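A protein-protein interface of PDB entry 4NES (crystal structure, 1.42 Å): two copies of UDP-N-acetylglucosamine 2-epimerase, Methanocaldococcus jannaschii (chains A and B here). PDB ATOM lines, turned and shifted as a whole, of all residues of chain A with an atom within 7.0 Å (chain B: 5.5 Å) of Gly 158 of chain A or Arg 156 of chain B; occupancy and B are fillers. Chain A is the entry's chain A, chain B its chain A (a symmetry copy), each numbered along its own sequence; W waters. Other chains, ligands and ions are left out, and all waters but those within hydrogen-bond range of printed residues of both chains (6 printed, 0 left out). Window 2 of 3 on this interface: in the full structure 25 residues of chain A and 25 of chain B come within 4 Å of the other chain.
Water W3 bridges NH2 of Arg 156 of chain A (2.6 Å) and O of Gly 158 of chain B (2.8 Å). Water W5 bridges the guanidinium group of Arg 156 of chain B (2.6 Å) and the backbone carbonyl oxygen of Gly 158 of chain A (2.8 Å). Water W4 lies within hydrogen-bond range of the side-chain carboxylate of Glu 160 of chain A (2.8 Å) and the guanidinium group of Arg 125 of chain B (3.0 Å). Water W1 lies within hydrogen-bond range of O of Glu 157 of chain A (2.8 Å), O of Gly 158 of chain A (3.2 Å) and NH2 of Arg 125 of chain B (3.2 Å). Water W2 lies within hydrogen-bond range of NH1 of Arg 156 of chain A (2.9 Å) and O of Gly 158 of chain B (3.4 Å). Water W6 lies within hydrogen-bond range of NH1 of Arg 156 of chain B, NH2 of Arg 125 of chain B and O of Gly 158 of chain A.
ND1 of His 138 of chain A is in hydrogen-bond range of NH1 of Arg 125 of chain B (3.2 Å). NH2 of Arg 156 of chain A sits at hydrogen-bond distance from O of Gly 158 of chain B, at 2.5 Å. NH2 of Arg 156 of chain B lies within hydrogen-bond range of O of Gly 158 of chain A, at 2.5 Å.
Gly 158 of chain A touches just one residue of chain B: Arg 156. Of chain A, only Arg 156 (3.5 Å), Glu 157 (3.7 Å) and Gly 158 (2.5 Å) come within 4 Å of Arg 156 of chain B. Printed residues of chain B within 4 Å of Glu 157 of chain A: Arg 156 (3.7 Å) and Glu 157 (3.4 Å). Printed residues of chain A within 4 Å of Glu 157 of chain B: Arg 156 and Glu 157. Of the printed residues of chain A, Arg 125 of chain B touches His 138 (3.2 Å). Printed residues of chain A within 4 Å of Gly 158 of chain B: Arg 156 (2.5 Å). Of the printed residues of chain B, His 138 of chain A touches Arg 125. Leu 155 of chain B touches none of the printed residues of chain A. The nearest residue of chain B that does not touch Gly 158 of chain A is Glu 157 of chain B (4.2 Å). The nearest residue of chain A that does not touch Arg 156 of chain B is Ile 159 of chain A (4.6 Å).
Among the printed residues, pairs that only touch across the chains: Arg 156 of chain A with Arg 156 of chain B (3.5 Å), Arg 156 of chain A with Glu 157 of chain B (3.7 Å), Glu 157 of chain A with Arg 156 of chain B (3.7 Å) and Glu 157 of chain A with Glu 157 of chain B (3.4 Å).
Arg 156 of chain B touches its own counterpart, Arg 156 of chain A. Arg 156 of chain A touches Glu 157 of chain B, and with the chains exchanged Glu 157 of chain A touches Arg 156 of chain B. Arg 156 of chain A touches Gly 158 of chain B, and with the chains exchanged Gly 158 of chain A touches Arg 156 of chain B. Glu 157 of chain A touches its own counterpart, Glu 157 of chain B. Positions printed for both chains: 152, 153, 154, 155, 156, 157 and 158.
Printed residues of chain A that touch a printed residue of chain B: His 138, Arg 156, Glu 157 and Gly 158. Of the 10 printed residues of chain B, 4 touch a printed residue of chain A. Among the printed residues, 7 pairs touch across the chains.
The side-chain carboxylate (OE1) of Glu 157 of chain A lies within hydrogen-bond range of a ring nitrogen (NE2) of His 138 of chain A. The guanidinium group of Arg 125 of chain B lies within salt-bridge range of the side-chain carboxylate of Glu 157 of chain B, at 3.1 Å.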
ATOM      1  N   HIS A 138      10.773  15.875 -20.621  1.00  0.00           N
ATOM      2  CA  HIS A 138      10.651  16.597 -19.373  1.00  0.00           C
ATOM      3  C   HIS A 138       9.689  17.772 -19.395  1.00  0.00           C
ATOM      4  O   HIS A 138       9.442  18.381 -18.358  1.00  0.00           O
ATOM      5  CB  HIS A 138      12.030  17.013 -18.869  1.00  0.00           C
ATOM      6  CG  HIS A 138      12.784  15.883 -18.272  1.00  0.00           C
ATOM      7  ND1 HIS A 138      12.725  15.576 -16.935  1.00  0.00           N
ATOM      8  CD2 HIS A 138      13.568  14.930 -18.843  1.00  0.00           C
ATOM      9  CE1 HIS A 138      13.458  14.499 -16.692  1.00  0.00           C
ATOM     10  NE2 HIS A 138      13.978  14.092 -17.843  1.00  0.00           N
ATOM     11  N   ASN A 152      10.560   2.756 -17.821  1.00  0.00           N
ATOM     12  CA  ASN A 152      11.539   2.736 -16.743  1.00  0.00           C
ATOM     13  C   ASN A 152      12.594   3.832 -16.894  1.00  0.00           C
ATOM     14  O   ASN A 152      13.029   4.418 -15.895  1.00  0.00           O
ATOM     15  CB  ASN A 152      12.162   1.346 -16.604  1.00  0.00           C
ATOM     16  CG  ASN A 152      11.200   0.347 -16.001  1.00  0.00           C
ATOM     17  OD1 ASN A 152      10.292   0.720 -15.263  1.00  0.00           O
ATOM     18  ND2 ASN A 152      11.395  -0.926 -16.306  1.00  0.00           N
ATOM     19  N   ASN A 153      12.995   4.121 -18.128  1.00  0.00           N
ATOM     20  CA  ASN A 153      13.876   5.262 -18.392  1.00  0.00           C
ATOM     21  C   ASN A 153      13.281   6.562 -17.870  1.00  0.00           C
ATOM     22  O   ASN A 153      13.976   7.376 -17.236  1.00  0.00           O
ATOM     23  CB  ASN A 153      14.150   5.400 -19.888  1.00  0.00           C
ATOM     24  CG  ASN A 153      15.074   4.335 -20.412  1.00  0.00           C
ATOM     25  OD1 ASN A 153      15.783   3.665 -19.647  1.00  0.00           O
ATOM     26  ND2 ASN A 153      15.100   4.184 -21.725  1.00  0.00           N
ATOM     27  N   LEU A 154      11.997   6.768 -18.135  1.00  0.00           N
ATOM     28  CA  LEU A 154      11.313   7.967 -17.688  1.00  0.00           C
ATOM     29  C   LEU A 154      11.209   8.029 -16.164  1.00  0.00           C
ATOM     30  O   LEU A 154      11.456   9.078 -15.564  1.00  0.00           O
ATOM     31  CB  LEU A 154       9.924   8.037 -18.318  1.00  0.00           C
ATOM     32  CG  LEU A 154       9.978   8.177 -19.838  1.00  0.00           C
ATOM     33  CD1 LEU A 154       8.651   7.843 -20.481  1.00  0.00           C
ATOM     34  CD2 LEU A 154      10.397   9.593 -20.218  1.00  0.00           C
ATOM     35  N   LEU A 155      10.866   6.912 -15.532  1.00  0.00           N
ATOM     36  CA  LEU A 155      10.761   6.861 -14.070  1.00  0.00           C
ATOM     37  C   LEU A 155      12.103   7.181 -13.405  1.00  0.00           C
ATOM     38  O   LEU A 155      12.152   7.882 -12.389  1.00  0.00           O
ATOM     39  CB  LEU A 155      10.240   5.502 -13.597  1.00  0.00           C
ATOM     40  CG  LEU A 155       8.789   5.186 -13.955  1.00  0.00           C
ATOM     41  CD1 LEU A 155       8.462   3.747 -13.595  1.00  0.00           C
ATOM     42  CD2 LEU A 155       7.829   6.157 -13.270  1.00  0.00           C
ATOM     43  N   ARG A 156      13.190   6.699 -14.002  1.00  0.00           N
ATOM     44  CA  ARG A 156      14.537   6.924 -13.481  1.00  0.00           C
ATOM     45  C   ARG A 156      14.944   8.397 -13.569  1.00  0.00           C
ATOM     46  O   ARG A 156      15.843   8.850 -12.846  1.00  0.00           O
ATOM     47  CB  ARG A 156      15.540   6.055 -14.246  1.00  0.00           C
ATOM     48  CG  ARG A 156      16.877   5.891 -13.557  1.00  0.00           C
ATOM     49  CD  ARG A 156      17.973   5.543 -14.551  1.00  0.00           C
ATOM     50  NE  ARG A 156      19.161   6.365 -14.333  1.00  0.00           N
ATOM     51  CZ  ARG A 156      19.531   7.372 -15.118  1.00  0.00           C
ATOM     52  NH1 ARG A 156      18.823   7.681 -16.197  1.00  0.00           N
ATOM     53  NH2 ARG A 156      20.626   8.062 -14.833  1.00  0.00           N
ATOM     54  N   GLU A 157      14.290   9.151 -14.446  1.00  0.00           N
ATOM     55  CA  GLU A 157      14.519  10.590 -14.552  1.00  0.00           C
ATOM     56  C   GLU A 157      13.472  11.388 -13.775  1.00  0.00           C
ATOM     57  O   GLU A 157      13.335  12.600 -13.964  1.00  0.00           O
ATOM     58  CB  GLU A 157      14.581  11.029 -16.020  1.00  0.00           C
ATOM     59  CG  GLU A 157      15.752  10.409 -16.763  1.00  0.00           C
ATOM     60  CD  GLU A 157      15.762  10.713 -18.249  1.00  0.00           C
ATOM     61  OE1 GLU A 157      14.999  11.595 -18.705  1.00  0.00           O
ATOM     62  OE2 GLU A 157      16.555  10.062 -18.966  1.00  0.00           O
ATOM     63  N   GLY A 158      12.740  10.695 -12.905  1.00  0.00           N
ATOM     64  CA  GLY A 158      11.865  11.347 -11.948  1.00  0.00           C
ATOM     65  C   GLY A 158      10.523  11.799 -12.484  1.00  0.00           C
ATOM     66  O   GLY A 158       9.802  12.520 -11.808  1.00  0.00           O
ATOM     67  N   ILE A 159      10.176  11.377 -13.693  1.00  0.00           N
ATOM     68  CA  ILE A 159       8.898  11.759 -14.278  1.00  0.00           C
ATOM     69  C   ILE A 159       7.780  10.990 -13.589  1.00  0.00           C
ATOM     70  O   ILE A 159       7.921   9.808 -13.283  1.00  0.00           O
ATOM     71  CB  ILE A 159       8.911  11.528 -15.802  1.00  0.00           C
ATOM     72  CG1 ILE A 159       9.796  12.590 -16.461  1.00  0.00           C
ATOM     73  CG2 ILE A 159       7.501  11.578 -16.402  1.00  0.00           C
ATOM     74  CD1 ILE A 159      10.279  12.213 -17.830  1.00  0.00           C
ATOM     75  N   GLU A 160       6.677  11.680 -13.315  1.00  0.00           N
ATOM     76  CA  GLU A 160       5.566  11.094 -12.579  1.00  0.00           C
ATOM     77  C   GLU A 160       4.887   9.969 -13.360  1.00  0.00           C
ATOM     78  O   GLU A 160       4.596  10.104 -14.562  1.00  0.00           O
ATOM     79  CB  GLU A 160       4.553  12.177 -12.206  1.00  0.00           C
ATOM     80  CG  GLU A 160       4.597  13.417 -13.094  1.00  0.00           C
ATOM     81  CD  GLU A 160       5.760  14.373 -12.798  1.00  0.00           C
ATOM     82  OE1 GLU A 160       5.813  14.948 -11.690  1.00  0.00           O
ATOM     83  OE2 GLU A 160       6.622  14.558 -13.684  1.00  0.00           O
ATOM     84  N   GLU A 161       4.638   8.855 -12.678  1.00  0.00           N
ATOM     85  CA  GLU A 161       4.108   7.680 -13.341  1.00  0.00           C
ATOM     86  C   GLU A 161       2.760   7.935 -14.008  1.00  0.00           C
ATOM     87  O   GLU A 161       2.454   7.327 -15.040  1.00  0.00           O
ATOM     88  CB  GLU A 161       4.010   6.492 -12.378  1.00  0.00           C
ATOM     89  CG  GLU A 161       3.674   5.180 -13.085  1.00  0.00           C
ATOM     90  CD  GLU A 161       3.896   3.958 -12.224  1.00  0.00           C
ATOM     91  OE1 GLU A 161       4.363   4.115 -11.076  1.00  0.00           O
ATOM     92  OE2 GLU A 161       3.603   2.838 -12.696  1.00  0.00           O
ATOM     93  N   PHE B 123       8.896  22.451  -8.288  1.00  0.00           N
ATOM     94  CA  PHE B 123       7.953  21.408  -8.716  1.00  0.00           C
ATOM     95  C   PHE B 123       6.627  21.981  -9.193  1.00  0.00           C
ATOM     96  O   PHE B 123       5.592  21.309  -9.187  1.00  0.00           O
ATOM     97  CB  PHE B 123       7.784  20.336  -7.636  1.00  0.00           C
ATOM     98  CG  PHE B 123       9.081  19.710  -7.230  1.00  0.00           C
ATOM     99  CD1 PHE B 123       9.776  18.897  -8.112  1.00  0.00           C
ATOM    100  CD2 PHE B 123       9.627  19.964  -5.985  1.00  0.00           C
ATOM    101  CE1 PHE B 123      10.987  18.332  -7.746  1.00  0.00           C
ATOM    102  CE2 PHE B 123      10.840  19.405  -5.611  1.00  0.00           C
ATOM    103  CZ  PHE B 123      11.514  18.581  -6.498  1.00  0.00           C
ATOM    104  N   ARG B 125       6.329  22.778 -12.351  1.00  0.00           N
ATOM    105  CA  ARG B 125       6.928  22.699 -13.692  1.00  0.00           C
ATOM    106  C   ARG B 125       6.028  23.313 -14.773  1.00  0.00           C
ATOM    107  O   ARG B 125       6.273  23.163 -15.972  1.00  0.00           O
ATOM    108  CB  ARG B 125       7.376  21.265 -14.042  1.00  0.00           C
ATOM    109  CG  ARG B 125       8.582  21.204 -14.994  1.00  0.00           C
ATOM    110  CD  ARG B 125       9.101  19.777 -15.260  1.00  0.00           C
ATOM    111  NE  ARG B 125       9.987  19.292 -14.199  1.00  0.00           N
ATOM    112  CZ  ARG B 125      10.664  18.146 -14.242  1.00  0.00           C
ATOM    113  NH1 ARG B 125      10.571  17.349 -15.305  1.00  0.00           N
ATOM    114  NH2 ARG B 125      11.441  17.801 -13.219  1.00  0.00           N
ATOM    115  N   LYS B 151      21.365  19.033  -5.063  1.00  0.00           N
ATOM    116  CA  LYS B 151      22.056  17.846  -5.572  1.00  0.00           C
ATOM    117  C   LYS B 151      21.121  16.646  -5.601  1.00  0.00           C
ATOM    118  O   LYS B 151      21.069  15.906  -6.583  1.00  0.00           O
ATOM    119  CB  LYS B 151      23.297  17.525  -4.739  1.00  0.00           C
ATOM    120  CG  LYS B 151      23.870  16.154  -5.066  1.00  0.00           C
ATOM    121  CD  LYS B 151      25.248  15.968  -4.481  1.00  0.00           C
ATOM    122  CE  LYS B 151      25.789  14.574  -4.810  1.00  0.00           C
ATOM    123  NZ  LYS B 151      27.176  14.389  -4.287  1.00  0.00           N
ATOM    124  N   ASN B 152      20.369  16.458  -4.527  1.00  0.00           N
ATOM    125  CA  ASN B 152      19.441  15.336  -4.466  1.00  0.00           C
ATOM    126  C   ASN B 152      18.332  15.440  -5.512  1.00  0.00           C
ATOM    127  O   ASN B 152      17.916  14.424  -6.082  1.00  0.00           O
ATOM    128  CB  ASN B 152      18.890  15.165  -3.050  1.00  0.00           C
ATOM    129  CG  ASN B 152      19.924  14.604  -2.099  1.00  0.00           C
ATOM    130  OD1 ASN B 152      20.848  13.910  -2.516  1.00  0.00           O
ATOM    131  ND2 ASN B 152      19.774  14.898  -0.817  1.00  0.00           N
ATOM    132  N   ASN B 153      17.861  16.655  -5.777  1.00  0.00           N
ATOM    133  CA  ASN B 153      16.917  16.880  -6.875  1.00  0.00           C
ATOM    134  C   ASN B 153      17.475  16.389  -8.204  1.00  0.00           C
ATOM    135  O   ASN B 153      16.773  15.726  -8.987  1.00  0.00           O
ATOM    136  CB  ASN B 153      16.568  18.363  -6.994  1.00  0.00           C
ATOM    137  CG  ASN B 153      15.671  18.841  -5.885  1.00  0.00           C
ATOM    138  OD1 ASN B 153      15.031  18.043  -5.186  1.00  0.00           O
ATOM    139  ND2 ASN B 153      15.592  20.151  -5.727  1.00  0.00           N
ATOM    140  N   LEU B 154      18.735  16.714  -8.467  1.00  0.00           N
ATOM    141  CA  LEU B 154      19.383  16.302  -9.698  1.00  0.00           C
ATOM    142  C   LEU B 154      19.553  14.785  -9.771  1.00  0.00           C
ATOM    143  O   LEU B 154      19.286  14.176 -10.811  1.00  0.00           O
ATOM    144  CB  LEU B 154      20.736  16.996  -9.829  1.00  0.00           C
ATOM    145  CG  LEU B 154      20.606  18.512  -9.960  1.00  0.00           C
ATOM    146  CD1 LEU B 154      21.916  19.214  -9.685  1.00  0.00           C
ATOM    147  CD2 LEU B 154      20.105  18.875 -11.353  1.00  0.00           C
ATOM    148  N   LEU B 155      19.977  14.167  -8.674  1.00  0.00           N
ATOM    149  CA  LEU B 155      20.150  12.711  -8.635  1.00  0.00           C
ATOM    150  C   LEU B 155      18.827  11.985  -8.895  1.00  0.00           C
ATOM    151  O   LEU B 155      18.793  10.970  -9.598  1.00  0.00           O
ATOM    152  CB  LEU B 155      20.755  12.259  -7.303  1.00  0.00           C
ATOM    153  CG  LEU B 155      22.201  12.684  -7.052  1.00  0.00           C
ATOM    154  CD1 LEU B 155      22.610  12.336  -5.631  1.00  0.00           C
ATOM    155  CD2 LEU B 155      23.146  12.045  -8.069  1.00  0.00           C
ATOM    156  N   ARG B 156      17.737  12.531  -8.361  1.00  0.00           N
ATOM    157  CA  ARG B 156      16.407  11.948  -8.527  1.00  0.00           C
ATOM    158  C   ARG B 156      15.928  12.020  -9.979  1.00  0.00           C
ATOM    159  O   ARG B 156      15.044  11.258 -10.393  1.00  0.00           O
ATOM    160  CB  ARG B 156      15.411  12.664  -7.608  1.00  0.00           C
ATOM    161  CG  ARG B 156      14.116  11.914  -7.387  1.00  0.00           C
ATOM    162  CD  ARG B 156      12.992  12.855  -6.985  1.00  0.00           C
ATOM    163  NE  ARG B 156      11.779  12.584  -7.752  1.00  0.00           N
ATOM    164  CZ  ARG B 156      11.327  13.354  -8.738  1.00  0.00           C
ATOM    165  NH1 ARG B 156      11.970  14.465  -9.074  1.00  0.00           N
ATOM    166  NH2 ARG B 156      10.216  13.020  -9.378  1.00  0.00           N
ATOM    167  N   GLU B 157      16.506  12.929 -10.758  1.00  0.00           N
ATOM    168  CA  GLU B 157      16.206  13.027 -12.185  1.00  0.00           C
ATOM    169  C   GLU B 157      17.250  12.301 -13.033  1.00  0.00           C
ATOM    170  O   GLU B 157      17.322  12.499 -14.250  1.00  0.00           O
ATOM    171  CB  GLU B 157      16.056  14.491 -12.614  1.00  0.00           C
ATOM    172  CG  GLU B 157      14.882  15.179 -11.938  1.00  0.00           C
ATOM    173  CD  GLU B 157      14.790  16.663 -12.234  1.00  0.00           C
ATOM    174  OE1 GLU B 157      15.490  17.156 -13.148  1.00  0.00           O
ATOM    175  OE2 GLU B 157      13.996  17.341 -11.544  1.00  0.00           O
ATOM    176  N   GLY B 158      18.052  11.464 -12.378  1.00  0.00           N
ATOM    177  CA  GLY B 158      18.940  10.550 -13.075  1.00  0.00           C
ATOM    178  C   GLY B 158      20.233  11.149 -13.585  1.00  0.00           C
ATOM    179  O   GLY B 158      20.951  10.508 -14.342  1.00  0.00           O
HETATM  180  O   HOH W   1      11.457  14.650 -13.449  1.00  0.00           O
HETATM  181  O   HOH W   2      20.312   9.800 -17.557  1.00  0.00           O
HETATM  182  O   HOH W   3      22.878   8.619 -13.664  1.00  0.00           O
HETATM  183  O   HOH W   4       7.925  15.984 -15.702  1.00  0.00           O
HETATM  184  O   HOH W   5       7.996  11.750  -9.835  1.00  0.00           O
HETATM  185  O   HOH W   6      10.324  15.760 -11.116  1.00  0.00           O
